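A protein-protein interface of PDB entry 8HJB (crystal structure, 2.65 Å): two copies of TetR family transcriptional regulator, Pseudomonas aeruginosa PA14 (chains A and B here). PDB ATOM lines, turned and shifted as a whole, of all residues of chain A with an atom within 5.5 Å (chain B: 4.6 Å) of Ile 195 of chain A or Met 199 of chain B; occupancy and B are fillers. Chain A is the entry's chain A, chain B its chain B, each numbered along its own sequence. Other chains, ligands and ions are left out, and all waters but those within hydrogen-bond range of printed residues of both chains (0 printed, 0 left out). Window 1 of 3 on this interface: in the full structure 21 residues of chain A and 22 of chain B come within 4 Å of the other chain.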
ATOM      1  N   LEU A 165       7.527  -0.888 -26.498  1.00  0.00           N
ATOM      2  CA  LEU A 165       8.297   0.014 -25.653  1.00  0.00           C
ATOM      3  C   LEU A 165       7.526   0.480 -24.430  1.00  0.00           C
ATOM      4  O   LEU A 165       8.105   0.584 -23.347  1.00  0.00           O
ATOM      5  CB  LEU A 165       8.763   1.232 -26.461  1.00  0.00           C
ATOM      6  CG  LEU A 165       9.505   2.321 -25.685  1.00  0.00           C
ATOM      7  CD1 LEU A 165      10.809   1.772 -25.126  1.00  0.00           C
ATOM      8  CD2 LEU A 165       9.767   3.537 -26.557  1.00  0.00           C
ATOM      9  N   HIS A 190      10.693  11.976 -19.711  1.00  0.00           N
ATOM     10  CA  HIS A 190      10.730  12.745 -20.949  1.00  0.00           C
ATOM     11  C   HIS A 190      11.757  12.183 -21.922  1.00  0.00           C
ATOM     12  O   HIS A 190      11.598  12.329 -23.139  1.00  0.00           O
ATOM     13  CB  HIS A 190      11.010  14.216 -20.646  1.00  0.00           C
ATOM     14  CG  HIS A 190       9.776  15.013 -20.359  1.00  0.00           C
ATOM     15  ND1 HIS A 190       8.867  14.650 -19.388  1.00  0.00           N
ATOM     16  CD2 HIS A 190       9.293  16.144 -20.923  1.00  0.00           C
ATOM     17  CE1 HIS A 190       7.879  15.526 -19.365  1.00  0.00           C
ATOM     18  NE2 HIS A 190       8.114  16.444 -20.285  1.00  0.00           N
ATOM     19  N   PHE A 191      12.804  11.535 -21.409  1.00  0.00           N
ATOM     20  CA  PHE A 191      13.746  10.853 -22.288  1.00  0.00           C
ATOM     21  C   PHE A 191      13.091   9.656 -22.966  1.00  0.00           C
ATOM     22  O   PHE A 191      13.347   9.386 -24.145  1.00  0.00           O
ATOM     23  CB  PHE A 191      14.980  10.425 -21.496  1.00  0.00           C
ATOM     24  CG  PHE A 191      16.094   9.900 -22.349  1.00  0.00           C
ATOM     25  CD1 PHE A 191      16.938  10.769 -23.018  1.00  0.00           C
ATOM     26  CD2 PHE A 191      16.305   8.538 -22.474  1.00  0.00           C
ATOM     27  CE1 PHE A 191      17.965  10.291 -23.806  1.00  0.00           C
ATOM     28  CE2 PHE A 191      17.334   8.052 -23.260  1.00  0.00           C
ATOM     29  CZ  PHE A 191      18.165   8.930 -23.925  1.00  0.00           C
ATOM     30  N   LEU A 192      12.237   8.931 -22.237  1.00  0.00           N
ATOM     31  CA  LEU A 192      11.503   7.820 -22.834  1.00  0.00           C
ATOM     32  C   LEU A 192      10.521   8.310 -23.892  1.00  0.00           C
ATOM     33  O   LEU A 192      10.331   7.655 -24.923  1.00  0.00           O
ATOM     34  CB  LEU A 192      10.770   7.035 -21.746  1.00  0.00           C
ATOM     35  CG  LEU A 192      11.497   5.840 -21.128  1.00  0.00           C
ATOM     36  CD1 LEU A 192      10.518   4.958 -20.372  1.00  0.00           C
ATOM     37  CD2 LEU A 192      12.217   5.043 -22.202  1.00  0.00           C
ATOM     38  N   MET A 193       9.886   9.457 -23.648  1.00  0.00           N
ATOM     39  CA  MET A 193       8.963  10.030 -24.623  1.00  0.00           C
ATOM     40  C   MET A 193       9.691  10.484 -25.883  1.00  0.00           C
ATOM     41  O   MET A 193       9.211  10.252 -27.000  1.00  0.00           O
ATOM     42  CB  MET A 193       8.206  11.185 -23.973  1.00  0.00           C
ATOM     43  CG  MET A 193       6.829  10.796 -23.471  1.00  0.00           C
ATOM     44  SD  MET A 193       5.983  12.133 -22.619  1.00  0.00           S
ATOM     45  CE  MET A 193       7.317  12.824 -21.662  1.00  0.00           C
ATOM     46  N   ASP A 194      10.847  11.131 -25.727  1.00  0.00           N
ATOM     47  CA  ASP A 194      11.624  11.526 -26.896  1.00  0.00           C
ATOM     48  C   ASP A 194      12.088  10.313 -27.688  1.00  0.00           C
ATOM     49  O   ASP A 194      12.297  10.408 -28.902  1.00  0.00           O
ATOM     50  CB  ASP A 194      12.821  12.377 -26.472  1.00  0.00           C
ATOM     51  CG  ASP A 194      12.407  13.663 -25.790  1.00  0.00           C
ATOM     52  OD1 ASP A 194      11.232  14.061 -25.938  1.00  0.00           O
ATOM     53  OD2 ASP A 194      13.252  14.272 -25.101  1.00  0.00           O
ATOM     54  N   ILE A 195      12.251   9.167 -27.022  1.00  0.00           N
ATOM     55  CA  ILE A 195      12.578   7.934 -27.730  1.00  0.00           C
ATOM     56  C   ILE A 195      11.418   7.514 -28.624  1.00  0.00           C
ATOM     57  O   ILE A 195      11.603   7.217 -29.809  1.00  0.00           O
ATOM     58  CB  ILE A 195      12.947   6.822 -26.732  1.00  0.00           C
ATOM     59  CG1 ILE A 195      14.365   7.024 -26.200  1.00  0.00           C
ATOM     60  CG2 ILE A 195      12.814   5.453 -27.379  1.00  0.00           C
ATOM     61  CD1 ILE A 195      14.569   6.471 -24.812  1.00  0.00           C
ATOM     62  N   GLY A 196      10.203   7.495 -28.070  1.00  0.00           N
ATOM     63  CA  GLY A 196       9.053   7.042 -28.837  1.00  0.00           C
ATOM     64  C   GLY A 196       8.728   7.950 -30.009  1.00  0.00           C
ATOM     65  O   GLY A 196       8.335   7.480 -31.078  1.00  0.00           O
ATOM     66  N   VAL A 197       8.883   9.261 -29.822  1.00  0.00           N
ATOM     67  CA  VAL A 197       8.644  10.199 -30.916  1.00  0.00           C
ATOM     68  C   VAL A 197       9.683  10.004 -32.013  1.00  0.00           C
ATOM     69  O   VAL A 197       9.348   9.888 -33.199  1.00  0.00           O
ATOM     70  CB  VAL A 197       8.639  11.646 -30.391  1.00  0.00           C
ATOM     71  CG1 VAL A 197       8.883  12.630 -31.527  1.00  0.00           C
ATOM     72  CG2 VAL A 197       7.327  11.945 -29.691  1.00  0.00           C
ATOM     73  N   ARG A 198      10.958   9.957 -31.635  1.00  0.00           N
ATOM     74  CA  ARG A 198      12.031   9.712 -32.587  1.00  0.00           C
ATOM     75  C   ARG A 198      12.144   8.248 -32.984  1.00  0.00           C
ATOM     76  O   ARG A 198      13.000   7.910 -33.810  1.00  0.00           O
ATOM     77  CB  ARG A 198      13.366  10.194 -32.015  1.00  0.00           C
ATOM     78  CG  ARG A 198      13.593  11.685 -32.161  1.00  0.00           C
ATOM     79  CD  ARG A 198      14.898  12.108 -31.501  1.00  0.00           C
ATOM     80  NE  ARG A 198      16.038  11.335 -31.980  1.00  0.00           N
ATOM     81  CZ  ARG A 198      16.541  11.405 -33.207  1.00  0.00           C
ATOM     82  NH1 ARG A 198      16.042  12.227 -34.115  1.00  0.00           N
ATOM     83  NH2 ARG A 198      17.576  10.633 -33.528  1.00  0.00           N
ATOM     84  N   MET A 199      11.312   7.378 -32.419  1.00  0.00           N
ATOM     85  CA  MET A 199      11.359   5.963 -32.756  1.00  0.00           C
ATOM     86  C   MET A 199      10.914   5.748 -34.195  1.00  0.00           C
ATOM     87  O   MET A 199       9.874   6.257 -34.621  1.00  0.00           O
ATOM     88  CB  MET A 199      10.468   5.159 -31.810  1.00  0.00           C
ATOM     89  CG  MET A 199      11.106   3.878 -31.298  1.00  0.00           C
ATOM     90  SD  MET A 199       9.917   2.619 -30.787  1.00  0.00           S
ATOM     91  CE  MET A 199       8.662   3.616 -29.984  1.00  0.00           C
ATOM     92  N   LEU B 150      25.422   9.689 -28.933  1.00  0.00           N
ATOM     93  CA  LEU B 150      24.293   9.600 -28.021  1.00  0.00           C
ATOM     94  C   LEU B 150      24.108  10.916 -27.274  1.00  0.00           C
ATOM     95  O   LEU B 150      25.060  11.674 -27.064  1.00  0.00           O
ATOM     96  CB  LEU B 150      24.498   8.458 -27.025  1.00  0.00           C
ATOM     97  CG  LEU B 150      24.324   7.031 -27.546  1.00  0.00           C
ATOM     98  CD1 LEU B 150      24.573   6.024 -26.434  1.00  0.00           C
ATOM     99  CD2 LEU B 150      22.936   6.845 -28.131  1.00  0.00           C
ATOM    100  N   ALA B 161      16.250   2.308 -20.835  1.00  0.00           N
ATOM    101  CA  ALA B 161      15.431   2.306 -22.040  1.00  0.00           C
ATOM    102  C   ALA B 161      15.810   1.161 -22.968  1.00  0.00           C
ATOM    103  O   ALA B 161      14.944   0.606 -23.651  1.00  0.00           O
ATOM    104  CB  ALA B 161      15.560   3.644 -22.766  1.00  0.00           C
ATOM    105  N   ALA B 162      17.094   0.797 -23.009  1.00  0.00           N
ATOM    106  CA  ALA B 162      17.503  -0.362 -23.792  1.00  0.00           C
ATOM    107  C   ALA B 162      16.933  -1.644 -23.202  1.00  0.00           C
ATOM    108  O   ALA B 162      16.502  -2.535 -23.944  1.00  0.00           O
ATOM    109  CB  ALA B 162      19.028  -0.434 -23.872  1.00  0.00           C
ATOM    110  N   LEU B 165      13.133  -1.868 -24.259  1.00  0.00           N
ATOM    111  CA  LEU B 165      12.857  -2.262 -25.636  1.00  0.00           C
ATOM    112  C   LEU B 165      13.087  -3.755 -25.840  1.00  0.00           C
ATOM    113  O   LEU B 165      12.354  -4.406 -26.593  1.00  0.00           O
ATOM    114  CB  LEU B 165      13.721  -1.451 -26.601  1.00  0.00           C
ATOM    115  CG  LEU B 165      13.342  -1.569 -28.078  1.00  0.00           C
ATOM    116  CD1 LEU B 165      12.440  -0.420 -28.500  1.00  0.00           C
ATOM    117  CD2 LEU B 165      14.585  -1.636 -28.956  1.00  0.00           C
ATOM    118  N   ILE B 195      15.769   0.613 -34.554  1.00  0.00           N
ATOM    119  CA  ILE B 195      15.210   1.407 -33.457  1.00  0.00           C
ATOM    120  C   ILE B 195      16.142   1.391 -32.254  1.00  0.00           C
ATOM    121  O   ILE B 195      16.429   2.436 -31.656  1.00  0.00           O
ATOM    122  CB  ILE B 195      13.804   0.903 -33.075  1.00  0.00           C
ATOM    123  CG1 ILE B 195      12.741   1.402 -34.060  1.00  0.00           C
ATOM    124  CG2 ILE B 195      13.463   1.278 -31.639  1.00  0.00           C
ATOM    125  CD1 ILE B 195      11.719   0.352 -34.431  1.00  0.00           C
ATOM    126  N   GLY B 196      16.627   0.206 -31.873  1.00  0.00           N
ATOM    127  CA  GLY B 196      17.438   0.102 -30.673  1.00  0.00           C
ATOM    128  C   GLY B 196      18.745   0.867 -30.771  1.00  0.00           C
ATOM    129  O   GLY B 196      19.156   1.534 -29.821  1.00  0.00           O
ATOM    130  N   VAL B 197      19.411   0.782 -31.924  1.00  0.00           N
ATOM    131  CA  VAL B 197      20.685   1.472 -32.091  1.00  0.00           C
ATOM    132  C   VAL B 197      20.475   2.976 -32.202  1.00  0.00           C
ATOM    133  O   VAL B 197      21.294   3.763 -31.709  1.00  0.00           O
ATOM    134  CB  VAL B 197      21.429   0.907 -33.317  1.00  0.00           C
ATOM    135  CG1 VAL B 197      22.670   1.733 -33.628  1.00  0.00           C
ATOM    136  CG2 VAL B 197      21.794  -0.545 -33.082  1.00  0.00           C
ATOM    137  N   ARG B 198      19.379   3.405 -32.825  1.00  0.00           N
ATOM    138  CA  ARG B 198      19.102   4.822 -33.002  1.00  0.00           C
ATOM    139  C   ARG B 198      18.370   5.447 -31.821  1.00  0.00           C
ATOM    140  O   ARG B 198      18.250   6.675 -31.769  1.00  0.00           O
ATOM    141  CB  ARG B 198      18.286   5.044 -34.278  1.00  0.00           C
ATOM    142  CG  ARG B 198      18.997   4.616 -35.549  1.00  0.00           C
ATOM    143  CD  ARG B 198      18.391   5.287 -36.769  1.00  0.00           C
ATOM    144  NE  ARG B 198      17.582   4.356 -37.545  1.00  0.00           N
ATOM    145  CZ  ARG B 198      16.308   4.553 -37.857  1.00  0.00           C
ATOM    146  NH1 ARG B 198      15.664   5.646 -37.480  1.00  0.00           N
ATOM    147  NH2 ARG B 198      15.664   3.628 -38.564  1.00  0.00           N
ATOM    148  N   MET B 199      17.884   4.646 -30.877  1.00  0.00           N
ATOM    149  CA  MET B 199      17.190   5.197 -29.721  1.00  0.00           C
ATOM    150  C   MET B 199      18.193   5.838 -28.768  1.00  0.00           C
ATOM    151  O   MET B 199      19.228   5.246 -28.447  1.00  0.00           O
ATOM    152  CB  MET B 199      16.389   4.108 -29.005  1.00  0.00           C
ATOM    153  CG  MET B 199      16.359   4.231 -27.490  1.00  0.00           C
ATOM    154  SD  MET B 199      15.379   2.931 -26.715  1.00  0.00           S
ATOM    155  CE  MET B 199      16.004   1.487 -27.566  1.00  0.00           C
ATOM    156  N   GLY B 200      17.885   7.054 -28.325  1.00  0.00           N
ATOM    157  CA  GLY B 200      18.764   7.791 -27.445  1.00  0.00           C
ATOM    158  C   GLY B 200      19.834   8.604 -28.137  1.00  0.00           C
ATOM    159  O   GLY B 200      20.650   9.233 -27.450  1.00  0.00           O
ATOM    160  N   ASN B 201      19.862   8.615 -29.468  1.00  0.00           N
ATOM    161  CA  ASN B 201      20.856   9.393 -30.191  1.00  0.00           C
ATOM    162  C   ASN B 201      20.640  10.886 -29.958  1.00  0.00           C
ATOM    163  O   ASN B 201      19.553  11.338 -29.588  1.00  0.00           O
ATOM    164  CB  ASN B 201      20.801   9.082 -31.688  1.00  0.00           C
ATOM    165  CG  ASN B 201      21.330   7.701 -32.019  1.00  0.00           C
ATOM    166  OD1 ASN B 201      21.810   6.981 -31.144  1.00  0.00           O
ATOM    167  ND2 ASN B 201      21.253   7.326 -33.290  1.00  0.00           N
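Among the printed residues, pairs that only touch across the chains: Phe 191 of chain A with Gly 200 of chain B, Leu 192 of chain A with Ala 161 of chain B, Ile 195 of chain A with Ala 161 of chain B, Ile 195 of chain A with Met 199 of chain B and Met 199 of chain A with Ile 195 of chain B.
Ile 195 of chain A touches Met 199 of chain B, and with the chains exchanged Met 199 of chain A touches Ile 195 of chain B.
Of the 5 pairs that touch across the chains among the printed residues, 2 have their exchanged pair printed and touching as well.
Ile 195 of chain A touches just these residues of chain B: Ala 161 (3.6 Å) and Met 199 (3.7 Å).
Met 199 of chain B touches just one residue of chain A: Ile 195 (3.7 Å).
Of the printed residues of chain A, Ala 161 of chain B touches Leu 192 and Ile 195.
Of the printed residues of chain B, Met 199 of chain A touches Ile 195.
Of the printed residues of chain A, Ile 195 of chain B touches Met 199.
Printed residues of chain B within 4 Å of Leu 192 of chain A: Ala 161.
Of the printed residues of chain B, Phe 191 of chain A touches Gly 200 (3.7 Å).
The nearest residue of chain B that does not touch Ile 195 of chain A is Gly 200 of chain B (4.1 Å).
The nearest residue of chain A that does not touch Met 199 of chain B is Leu 165 of chain A (5.0 Å).
The nearest printed residue of chain A that does not touch Gly 200 of chain B is Ile 195 of chain A (4.1 Å).
Hydrophobic or aromatic side chains of chain B that line the printed part of chain A: Ala 161, Ile 195 and Met 199.
Of the 11 printed residues of chain A, 4 touch a printed residue of chain B.
Among the printed residues, 5 pairs touch across the chains.
Among the printed residues, no Asp or Glu carboxylate lies within 4 Å of a Lys or Arg side-chain nitrogen of the other chain.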
